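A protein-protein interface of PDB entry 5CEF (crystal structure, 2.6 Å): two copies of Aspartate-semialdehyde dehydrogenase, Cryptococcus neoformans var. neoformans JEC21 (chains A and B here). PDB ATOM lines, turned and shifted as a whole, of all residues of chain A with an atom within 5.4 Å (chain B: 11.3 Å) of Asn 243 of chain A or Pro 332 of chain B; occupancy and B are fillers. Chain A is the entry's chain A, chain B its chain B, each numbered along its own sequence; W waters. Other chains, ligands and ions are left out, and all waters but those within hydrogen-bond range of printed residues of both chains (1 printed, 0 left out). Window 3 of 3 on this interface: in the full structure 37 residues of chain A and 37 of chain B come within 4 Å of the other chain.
The side-chain amino group of Lys 337 of chain B lies within salt-bridge range of the side-chain carboxylate of Glu 217 of chain A (2.8 Å). OD1 of Asn 243 of chain A sits close to O of Pro 332 of chain B, at 2.9 Å. SG of Cys 331 of chain B sits at hydrogen-bond distance from OG of Ser 245 of chain A (3.0 Å). The side-chain amino group (NZ) of Lys 337 of chain B lies within hydrogen-bond range of the side-chain hydroxyl (OG) of Ser 245 of chain A (3.0 Å).
The side-chain carboxylate of Asp 178 of chain A sits at hydrogen-bond distance from the side-chain hydroxyl of Thr 179 of chain A (3.0 Å). The backbone carbonyl oxygen (O) of Asp 178 of chain A is in hydrogen-bond range of the backbone NH (N) of Asn 243 of chain A (2.9 Å). N of Val 180 of chain A is in hydrogen-bond range of O of Asn 243 of chain A (2.8 Å). O of Val 180 of chain A is in hydrogen-bond range of N of Ser 245 of chain A (3.0 Å). O of Arg 329 of chain B lies within hydrogen-bond range of N of Lys 337 of chain B (2.9 Å). SG of Cys 331 of chain B sits close to N of Val 333 of chain B (3.5 Å).
Among the printed residues, merely in contact across the chains: Thr 179 of chain A with Val 333 of chain B (3.6 Å), Ile 181 of chain A with Ile 181 of chain B (3.9 Å), Ile 181 of chain A with Phe 334 of chain B (3.4 Å), Glu 217 of chain A with Pro 332 of chain B (3.8 Å), Asn 243 of chain A with Val 333 of chain B (3.6 Å), Val 244 of chain A with Pro 332 of chain B (3.6 Å), Val 244 of chain A with Val 333 of chain B (3.9 Å), Ser 245 of chain A with Pro 332 of chain B (3.8 Å) and Ser 245 of chain A with Val 333 of chain B (3.6 Å).
Asn 243 of chain A touches two residues of chain B. Pro 332 of chain B touches just these residues of chain A: Glu 217 (3.8 Å), Asn 243 (2.9 Å), Val 244 (3.6 Å) and Ser 245 (3.8 Å). No residue of chain B comes within 4 Å of Asp 178 of chain A. No residue of chain B comes within 4 Å of Val 180 of chain A. No residue of chain B comes within 4 Å of Ile 242 of chain A. Printed residues of chain A within 4 Å of Cys 331 of chain B: Ser 245. Printed residues of chain A within 4 Å of Val 333 of chain B: Thr 179, Asn 243, Val 244 and Ser 245. Printed residues of chain B within 4 Å of Glu 217 of chain A: Pro 332 (3.8 Å) and Lys 337 (2.8 Å). Printed residues of chain A within 4 Å of Ile 181 of chain B: Ile 181. The nearest residue of chain B that does not touch Asn 243 of chain A is Phe 334 of chain B (6.4 Å). The nearest printed residue of chain A that does not touch Pro 332 of chain B is Ile 242 of chain A (7.4 Å). The nearest printed residue of chain A that does not touch Phe 334 of chain B is Ser 245 of chain A (5.9 Å).
Of the 19 printed residues of chain B, 6 touch a printed residue of chain A. Hydrophobic or aromatic side chains of chain B that line the printed part of chain A: Ile 181, Pro 332, Val 333 and Phe 334. Of the 11 printed residues of chain A, 6 touch a printed residue of chain B. Printed residues of chain A that touch a printed residue of chain B: Thr 179, Ile 181, Glu 217, Asn 243, Val 244 and Ser 245. Hydrophobic or aromatic side chains of chain A within 4 Å of the printed part of chain B: Ile 181.
Ile 181 of chain A touches its own counterpart, Ile 181 of chain B.
Water W1 bridges OE1 of Glu 217 of chain A (2.7 Å) and NZ of Lys 337 of chain B (2.7 Å).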
ATOM      1  N   ASP A 178     -15.624  31.903 -38.691  1.00  0.00           N
ATOM      2  CA  ASP A 178     -15.130  31.888 -37.337  1.00  0.00           C
ATOM      3  C   ASP A 178     -15.904  30.863 -36.537  1.00  0.00           C
ATOM      4  O   ASP A 178     -15.334  29.938 -35.975  1.00  0.00           O
ATOM      5  CB  ASP A 178     -15.353  33.305 -36.768  1.00  0.00           C
ATOM      6  CG  ASP A 178     -15.011  33.458 -35.306  1.00  0.00           C
ATOM      7  OD1 ASP A 178     -14.627  32.501 -34.619  1.00  0.00           O
ATOM      8  OD2 ASP A 178     -15.082  34.603 -34.839  1.00  0.00           O
ATOM      9  N   THR A 179     -17.216  31.042 -36.487  1.00  0.00           N
ATOM     10  CA  THR A 179     -18.089  30.313 -35.549  1.00  0.00           C
ATOM     11  C   THR A 179     -19.387  29.901 -36.235  1.00  0.00           C
ATOM     12  O   THR A 179     -19.936  30.652 -37.057  1.00  0.00           O
ATOM     13  CB  THR A 179     -18.403  31.198 -34.338  1.00  0.00           C
ATOM     14  OG1 THR A 179     -17.210  31.391 -33.561  1.00  0.00           O
ATOM     15  CG2 THR A 179     -19.451  30.596 -33.470  1.00  0.00           C
ATOM     16  N   VAL A 180     -19.828  28.683 -35.923  1.00  0.00           N
ATOM     17  CA  VAL A 180     -21.091  28.135 -36.396  1.00  0.00           C
ATOM     18  C   VAL A 180     -21.863  27.393 -35.313  1.00  0.00           C
ATOM     19  O   VAL A 180     -21.320  26.509 -34.651  1.00  0.00           O
ATOM     20  CB  VAL A 180     -20.875  27.142 -37.550  1.00  0.00           C
ATOM     21  CG1 VAL A 180     -22.215  26.541 -37.985  1.00  0.00           C
ATOM     22  CG2 VAL A 180     -20.203  27.810 -38.750  1.00  0.00           C
ATOM     23  N   ILE A 181     -23.135  27.734 -35.153  1.00  0.00           N
ATOM     24  CA  ILE A 181     -24.029  27.025 -34.235  1.00  0.00           C
ATOM     25  C   ILE A 181     -25.183  26.502 -35.024  1.00  0.00           C
ATOM     26  O   ILE A 181     -25.711  27.193 -35.895  1.00  0.00           O
ATOM     27  CB  ILE A 181     -24.533  27.924 -33.089  1.00  0.00           C
ATOM     28  CG1 ILE A 181     -23.359  28.212 -32.154  1.00  0.00           C
ATOM     29  CG2 ILE A 181     -25.642  27.255 -32.307  1.00  0.00           C
ATOM     30  CD1 ILE A 181     -23.742  28.565 -30.746  1.00  0.00           C
ATOM     31  N   GLU A 217     -19.371  18.371 -35.796  1.00  0.00           N
ATOM     32  CA  GLU A 217     -18.404  19.271 -35.130  1.00  0.00           C
ATOM     33  C   GLU A 217     -16.978  19.043 -35.566  1.00  0.00           C
ATOM     34  O   GLU A 217     -16.230  19.982 -35.779  1.00  0.00           O
ATOM     35  CB  GLU A 217     -18.525  19.158 -33.598  1.00  0.00           C
ATOM     36  CG  GLU A 217     -19.814  19.804 -33.083  1.00  0.00           C
ATOM     37  CD  GLU A 217     -20.096  19.615 -31.602  1.00  0.00           C
ATOM     38  OE1 GLU A 217     -19.266  18.990 -30.925  1.00  0.00           O
ATOM     39  OE2 GLU A 217     -21.117  20.125 -31.130  1.00  0.00           O
ATOM     40  N   ASN A 221     -14.552  20.860 -40.202  1.00  0.00           N
ATOM     41  CA  ASN A 221     -13.221  21.478 -40.388  1.00  0.00           C
ATOM     42  C   ASN A 221     -12.343  20.714 -41.348  1.00  0.00           C
ATOM     43  O   ASN A 221     -11.663  21.297 -42.206  1.00  0.00           O
ATOM     44  CB  ASN A 221     -12.524  21.687 -39.055  1.00  0.00           C
ATOM     45  CG  ASN A 221     -12.908  23.024 -38.393  1.00  0.00           C
ATOM     46  OD1 ASN A 221     -12.831  24.096 -39.009  1.00  0.00           O
ATOM     47  ND2 ASN A 221     -13.267  22.970 -37.163  1.00  0.00           N
ATOM     48  N   GLN A 241      -9.277  27.373 -36.928  1.00  0.00           N
ATOM     49  CA  GLN A 241     -10.342  26.407 -37.155  1.00  0.00           C
ATOM     50  C   GLN A 241     -11.703  27.028 -36.871  1.00  0.00           C
ATOM     51  O   GLN A 241     -11.834  27.861 -35.993  1.00  0.00           O
ATOM     52  CB  GLN A 241     -10.172  25.174 -36.252  1.00  0.00           C
ATOM     53  CG  GLN A 241      -8.986  24.339 -36.654  1.00  0.00           C
ATOM     54  CD  GLN A 241      -8.956  22.977 -35.977  1.00  0.00           C
ATOM     55  OE1 GLN A 241      -8.920  22.884 -34.767  1.00  0.00           O
ATOM     56  NE2 GLN A 241      -9.021  21.918 -36.771  1.00  0.00           N
ATOM     57  N   ILE A 242     -12.716  26.568 -37.581  1.00  0.00           N
ATOM     58  CA  ILE A 242     -14.094  26.975 -37.313  1.00  0.00           C
ATOM     59  C   ILE A 242     -14.549  26.386 -35.978  1.00  0.00           C
ATOM     60  O   ILE A 242     -14.378  25.218 -35.722  1.00  0.00           O
ATOM     61  CB  ILE A 242     -15.071  26.466 -38.413  1.00  0.00           C
ATOM     62  CG1 ILE A 242     -14.636  26.941 -39.800  1.00  0.00           C
ATOM     63  CG2 ILE A 242     -16.471  26.969 -38.133  1.00  0.00           C
ATOM     64  CD1 ILE A 242     -15.413  26.259 -40.914  1.00  0.00           C
ATOM     65  N   ASN A 243     -15.166  27.191 -35.153  1.00  0.00           N
ATOM     66  CA  ASN A 243     -15.797  26.701 -33.954  1.00  0.00           C
ATOM     67  C   ASN A 243     -17.218  26.284 -34.194  1.00  0.00           C
ATOM     68  O   ASN A 243     -18.064  27.135 -34.478  1.00  0.00           O
ATOM     69  CB  ASN A 243     -15.831  27.801 -32.948  1.00  0.00           C
ATOM     70  CG  ASN A 243     -14.742  27.647 -31.958  1.00  0.00           C
ATOM     71  OD1 ASN A 243     -14.935  27.000 -30.891  1.00  0.00           O
ATOM     72  ND2 ASN A 243     -13.571  28.178 -32.298  1.00  0.00           N
ATOM     73  N   VAL A 244     -17.491  24.995 -34.035  1.00  0.00           N
ATOM     74  CA  VAL A 244     -18.790  24.460 -34.349  1.00  0.00           C
ATOM     75  C   VAL A 244     -19.453  23.806 -33.148  1.00  0.00           C
ATOM     76  O   VAL A 244     -18.829  23.012 -32.451  1.00  0.00           O
ATOM     77  CB  VAL A 244     -18.704  23.416 -35.492  1.00  0.00           C
ATOM     78  CG1 VAL A 244     -20.106  23.034 -35.949  1.00  0.00           C
ATOM     79  CG2 VAL A 244     -17.937  23.963 -36.684  1.00  0.00           C
ATOM     80  N   SER A 245     -20.729  24.143 -32.922  1.00  0.00           N
ATOM     81  CA  SER A 245     -21.504  23.494 -31.866  1.00  0.00           C
ATOM     82  C   SER A 245     -22.846  23.106 -32.429  1.00  0.00           C
ATOM     83  O   SER A 245     -23.584  23.961 -32.920  1.00  0.00           O
ATOM     84  CB  SER A 245     -21.678  24.445 -30.688  1.00  0.00           C
ATOM     85  OG  SER A 245     -22.373  23.867 -29.622  1.00  0.00           O
ATOM     86  N   ILE B 181     -28.086  31.355 -27.309  1.00  0.00           N
ATOM     87  CA  ILE B 181     -28.600  30.981 -28.596  1.00  0.00           C
ATOM     88  C   ILE B 181     -29.598  29.837 -28.399  1.00  0.00           C
ATOM     89  O   ILE B 181     -29.319  28.892 -27.688  1.00  0.00           O
ATOM     90  CB  ILE B 181     -27.455  30.580 -29.560  1.00  0.00           C
ATOM     91  CG1 ILE B 181     -26.667  31.839 -29.916  1.00  0.00           C
ATOM     92  CG2 ILE B 181     -28.013  29.952 -30.842  1.00  0.00           C
ATOM     93  CD1 ILE B 181     -25.925  31.778 -31.234  1.00  0.00           C
ATOM     94  N   VAL B 261     -30.493  24.830 -26.429  1.00  0.00           N
ATOM     95  CA  VAL B 261     -29.989  26.084 -25.896  1.00  0.00           C
ATOM     96  C   VAL B 261     -28.483  26.034 -25.671  1.00  0.00           C
ATOM     97  O   VAL B 261     -27.976  25.047 -25.111  1.00  0.00           O
ATOM     98  CB  VAL B 261     -30.684  26.416 -24.543  1.00  0.00           C
ATOM     99  CG1 VAL B 261     -30.237  27.790 -24.021  1.00  0.00           C
ATOM    100  CG2 VAL B 261     -32.194  26.429 -24.708  1.00  0.00           C
ATOM    101  N   SER B 262     -27.775  27.080 -26.089  1.00  0.00           N
ATOM    102  CA  SER B 262     -26.367  27.236 -25.737  1.00  0.00           C
ATOM    103  C   SER B 262     -26.175  28.505 -24.931  1.00  0.00           C
ATOM    104  O   SER B 262     -26.747  29.535 -25.264  1.00  0.00           O
ATOM    105  CB  SER B 262     -25.477  27.268 -26.988  1.00  0.00           C
ATOM    106  OG  SER B 262     -25.633  26.070 -27.757  1.00  0.00           O
ATOM    107  N   VAL B 263     -25.374  28.424 -23.873  1.00  0.00           N
ATOM    108  CA  VAL B 263     -25.220  29.537 -22.954  1.00  0.00           C
ATOM    109  C   VAL B 263     -23.760  29.859 -22.708  1.00  0.00           C
ATOM    110  O   VAL B 263     -22.929  28.960 -22.493  1.00  0.00           O
ATOM    111  CB  VAL B 263     -25.864  29.221 -21.617  1.00  0.00           C
ATOM    112  CG1 VAL B 263     -25.652  30.344 -20.645  1.00  0.00           C
ATOM    113  CG2 VAL B 263     -27.351  29.026 -21.811  1.00  0.00           C
ATOM    114  N   LYS B 264     -23.457  31.154 -22.723  1.00  0.00           N
ATOM    115  CA  LYS B 264     -22.167  31.664 -22.238  1.00  0.00           C
ATOM    116  C   LYS B 264     -22.399  32.487 -20.986  1.00  0.00           C
ATOM    117  O   LYS B 264     -23.122  33.469 -21.033  1.00  0.00           O
ATOM    118  CB  LYS B 264     -21.528  32.552 -23.295  1.00  0.00           C
ATOM    119  CG  LYS B 264     -20.329  33.330 -22.817  1.00  0.00           C
ATOM    120  CD  LYS B 264     -19.031  32.739 -23.350  1.00  0.00           C
ATOM    121  CE  LYS B 264     -17.907  32.756 -22.303  1.00  0.00           C
ATOM    122  NZ  LYS B 264     -17.047  31.544 -22.424  1.00  0.00           N
ATOM    123  N   PRO B 270     -16.378  28.942 -16.125  1.00  0.00           N
ATOM    124  CA  PRO B 270     -17.768  28.512 -16.075  1.00  0.00           C
ATOM    125  C   PRO B 270     -17.908  27.255 -15.232  1.00  0.00           C
ATOM    126  O   PRO B 270     -16.924  26.526 -15.036  1.00  0.00           O
ATOM    127  CB  PRO B 270     -18.062  28.181 -17.531  1.00  0.00           C
ATOM    128  CG  PRO B 270     -16.754  27.622 -18.020  1.00  0.00           C
ATOM    129  CD  PRO B 270     -15.693  28.427 -17.328  1.00  0.00           C
ATOM    130  N   VAL B 273     -20.519  20.573 -15.697  1.00  0.00           N
ATOM    131  CA  VAL B 273     -21.760  19.886 -15.968  1.00  0.00           C
ATOM    132  C   VAL B 273     -22.473  19.533 -14.673  1.00  0.00           C
ATOM    133  O   VAL B 273     -23.665  19.768 -14.547  1.00  0.00           O
ATOM    134  CB  VAL B 273     -21.467  18.626 -16.802  1.00  0.00           C
ATOM    135  CG1 VAL B 273     -22.645  17.675 -16.816  1.00  0.00           C
ATOM    136  CG2 VAL B 273     -21.083  19.047 -18.218  1.00  0.00           C
ATOM    137  N   ARG B 327     -29.480  16.379 -21.493  1.00  0.00           N
ATOM    138  CA  ARG B 327     -28.318  16.511 -22.363  1.00  0.00           C
ATOM    139  C   ARG B 327     -27.493  17.723 -21.997  1.00  0.00           C
ATOM    140  O   ARG B 327     -26.981  18.437 -22.863  1.00  0.00           O
ATOM    141  CB  ARG B 327     -28.744  16.576 -23.819  1.00  0.00           C
ATOM    142  CG  ARG B 327     -29.631  15.413 -24.199  1.00  0.00           C
ATOM    143  CD  ARG B 327     -29.579  15.042 -25.688  1.00  0.00           C
ATOM    144  NE  ARG B 327     -28.219  14.844 -26.140  1.00  0.00           N
ATOM    145  CZ  ARG B 327     -27.664  15.429 -27.196  1.00  0.00           C
ATOM    146  NH1 ARG B 327     -28.351  16.204 -28.023  1.00  0.00           N
ATOM    147  NH2 ARG B 327     -26.405  15.200 -27.450  1.00  0.00           N
ATOM    148  N   ILE B 328     -27.280  17.917 -20.701  1.00  0.00           N
ATOM    149  CA  ILE B 328     -26.397  18.996 -20.254  1.00  0.00           C
ATOM    150  C   ILE B 328     -24.917  18.660 -20.473  1.00  0.00           C
ATOM    151  O   ILE B 328     -24.409  17.646 -19.983  1.00  0.00           O
ATOM    152  CB  ILE B 328     -26.610  19.301 -18.802  1.00  0.00           C
ATOM    153  CG1 ILE B 328     -28.033  19.800 -18.625  1.00  0.00           C
ATOM    154  CG2 ILE B 328     -25.610  20.334 -18.337  1.00  0.00           C
ATOM    155  CD1 ILE B 328     -28.551  19.577 -17.222  1.00  0.00           C
ATOM    156  N   ARG B 329     -24.238  19.497 -21.252  1.00  0.00           N
ATOM    157  CA  ARG B 329     -22.892  19.166 -21.698  1.00  0.00           C
ATOM    158  C   ARG B 329     -22.139  20.382 -22.147  1.00  0.00           C
ATOM    159  O   ARG B 329     -22.693  21.445 -22.372  1.00  0.00           O
ATOM    160  CB  ARG B 329     -22.954  18.107 -22.819  1.00  0.00           C
ATOM    161  CG  ARG B 329     -23.605  18.563 -24.120  1.00  0.00           C
ATOM    162  CD  ARG B 329     -24.347  17.449 -24.877  1.00  0.00           C
ATOM    163  NE  ARG B 329     -24.745  17.902 -26.217  1.00  0.00           N
ATOM    164  CZ  ARG B 329     -25.792  18.690 -26.509  1.00  0.00           C
ATOM    165  NH1 ARG B 329     -26.637  19.126 -25.572  1.00  0.00           N
ATOM    166  NH2 ARG B 329     -25.988  19.053 -27.769  1.00  0.00           N
ATOM    167  N   GLU B 330     -20.844  20.227 -22.303  1.00  0.00           N
ATOM    168  CA  GLU B 330     -20.021  21.345 -22.757  1.00  0.00           C
ATOM    169  C   GLU B 330     -20.377  21.740 -24.170  1.00  0.00           C
ATOM    170  O   GLU B 330     -20.658  20.874 -24.998  1.00  0.00           O
ATOM    171  CB  GLU B 330     -18.541  20.997 -22.665  1.00  0.00           C
ATOM    172  CG  GLU B 330     -18.026  21.127 -21.241  1.00  0.00           C
ATOM    173  CD  GLU B 330     -16.563  20.751 -21.124  1.00  0.00           C
ATOM    174  OE1 GLU B 330     -15.786  21.048 -22.075  1.00  0.00           O
ATOM    175  OE2 GLU B 330     -16.216  20.150 -20.089  1.00  0.00           O
ATOM    176  N   CYS B 331     -20.318  23.044 -24.428  1.00  0.00           N
ATOM    177  CA  CYS B 331     -20.448  23.617 -25.760  1.00  0.00           C
ATOM    178  C   CYS B 331     -19.067  24.064 -26.231  1.00  0.00           C
ATOM    179  O   CYS B 331     -18.437  24.902 -25.619  1.00  0.00           O
ATOM    180  CB  CYS B 331     -21.378  24.827 -25.725  1.00  0.00           C
ATOM    181  SG  CYS B 331     -21.658  25.661 -27.295  1.00  0.00           S
ATOM    182  N   PRO B 332     -18.595  23.525 -27.351  1.00  0.00           N
ATOM    183  CA  PRO B 332     -17.311  24.014 -27.901  1.00  0.00           C
ATOM    184  C   PRO B 332     -17.235  25.523 -28.215  1.00  0.00           C
ATOM    185  O   PRO B 332     -16.141  26.041 -28.406  1.00  0.00           O
ATOM    186  CB  PRO B 332     -17.167  23.202 -29.213  1.00  0.00           C
ATOM    187  CG  PRO B 332     -17.981  21.990 -28.998  1.00  0.00           C
ATOM    188  CD  PRO B 332     -19.163  22.444 -28.170  1.00  0.00           C
ATOM    189  N   VAL B 333     -18.383  26.198 -28.309  1.00  0.00           N
ATOM    190  CA  VAL B 333     -18.430  27.583 -28.721  1.00  0.00           C
ATOM    191  C   VAL B 333     -18.667  28.540 -27.558  1.00  0.00           C
ATOM    192  O   VAL B 333     -18.017  29.555 -27.458  1.00  0.00           O
ATOM    193  CB  VAL B 333     -19.526  27.795 -29.796  1.00  0.00           C
ATOM    194  CG1 VAL B 333     -19.700  29.280 -30.104  1.00  0.00           C
ATOM    195  CG2 VAL B 333     -19.156  27.055 -31.049  1.00  0.00           C
ATOM    196  N   PHE B 334     -19.626  28.217 -26.712  1.00  0.00           N
ATOM    197  CA  PHE B 334     -19.911  28.988 -25.504  1.00  0.00           C
ATOM    198  C   PHE B 334     -19.462  28.166 -24.278  1.00  0.00           C
ATOM    199  O   PHE B 334     -18.410  27.551 -24.333  1.00  0.00           O
ATOM    200  CB  PHE B 334     -21.404  29.325 -25.490  1.00  0.00           C
ATOM    201  CG  PHE B 334     -21.803  30.297 -26.559  1.00  0.00           C
ATOM    202  CD1 PHE B 334     -21.011  31.381 -26.857  1.00  0.00           C
ATOM    203  CD2 PHE B 334     -22.957  30.096 -27.297  1.00  0.00           C
ATOM    204  CE1 PHE B 334     -21.359  32.271 -27.867  1.00  0.00           C
ATOM    205  CE2 PHE B 334     -23.319  30.963 -28.306  1.00  0.00           C
ATOM    206  CZ  PHE B 334     -22.521  32.063 -28.586  1.00  0.00           C
ATOM    207  N   ASP B 335     -20.259  28.069 -23.218  1.00  0.00           N
ATOM    208  CA  ASP B 335     -19.859  27.283 -22.047  1.00  0.00           C
ATOM    209  C   ASP B 335     -20.626  26.000 -21.892  1.00  0.00           C
ATOM    210  O   ASP B 335     -20.041  24.940 -21.763  1.00  0.00           O
ATOM    211  CB  ASP B 335     -20.029  28.130 -20.780  1.00  0.00           C
ATOM    212  CG  ASP B 335     -19.101  29.314 -20.772  1.00  0.00           C
ATOM    213  OD1 ASP B 335     -17.950  29.121 -21.268  1.00  0.00           O
ATOM    214  OD2 ASP B 335     -19.502  30.409 -20.320  1.00  0.00           O
ATOM    215  N   ILE B 336     -21.944  26.096 -21.919  1.00  0.00           N
ATOM    216  CA  ILE B 336     -22.801  24.963 -21.648  1.00  0.00           C
ATOM    217  C   ILE B 336     -23.967  24.940 -22.632  1.00  0.00           C
ATOM    218  O   ILE B 336     -24.496  25.990 -22.980  1.00  0.00           O
ATOM    219  CB  ILE B 336     -23.276  25.053 -20.194  1.00  0.00           C
ATOM    220  CG1 ILE B 336     -22.232  24.404 -19.266  1.00  0.00           C
ATOM    221  CG2 ILE B 336     -24.687  24.525 -20.015  1.00  0.00           C
ATOM    222  CD1 ILE B 336     -22.161  22.902 -19.280  1.00  0.00           C
ATOM    223  N   LYS B 337     -24.341  23.743 -23.091  1.00  0.00           N
ATOM    224  CA  LYS B 337     -25.560  23.579 -23.876  1.00  0.00           C
ATOM    225  C   LYS B 337     -26.452  22.462 -23.338  1.00  0.00           C
ATOM    226  O   LYS B 337     -25.988  21.555 -22.626  1.00  0.00           O
ATOM    227  CB  LYS B 337     -25.264  23.384 -25.370  1.00  0.00           C
ATOM    228  CG  LYS B 337     -24.415  22.170 -25.740  1.00  0.00           C
ATOM    229  CD  LYS B 337     -24.126  22.154 -27.241  1.00  0.00           C
ATOM    230  CE  LYS B 337     -23.165  21.016 -27.582  1.00  0.00           C
ATOM    231  NZ  LYS B 337     -22.715  20.933 -29.007  1.00  0.00           N
ATOM    232  N   PHE B 338     -27.738  22.537 -23.682  1.00  0.00           N
ATOM    233  CA  PHE B 338     -28.689  21.600 -23.140  1.00  0.00           C
ATOM    234  C   PHE B 338     -29.972  21.612 -23.918  1.00  0.00           C
ATOM    235  O   PHE B 338     -30.155  22.392 -24.842  1.00  0.00           O
ATOM    236  CB  PHE B 338     -28.968  21.875 -21.648  1.00  0.00           C
ATOM    237  CG  PHE B 338     -29.579  23.219 -21.374  1.00  0.00           C
ATOM    238  CD1 PHE B 338     -28.784  24.319 -21.186  1.00  0.00           C
ATOM    239  CD2 PHE B 338     -30.933  23.367 -21.267  1.00  0.00           C
ATOM    240  CE1 PHE B 338     -29.329  25.567 -20.939  1.00  0.00           C
ATOM    241  CE2 PHE B 338     -31.491  24.610 -21.030  1.00  0.00           C
ATOM    242  CZ  PHE B 338     -30.686  25.722 -20.870  1.00  0.00           C
HETATM  243  O   HOH W   1     -20.606  19.237 -28.562  1.00  0.00           O
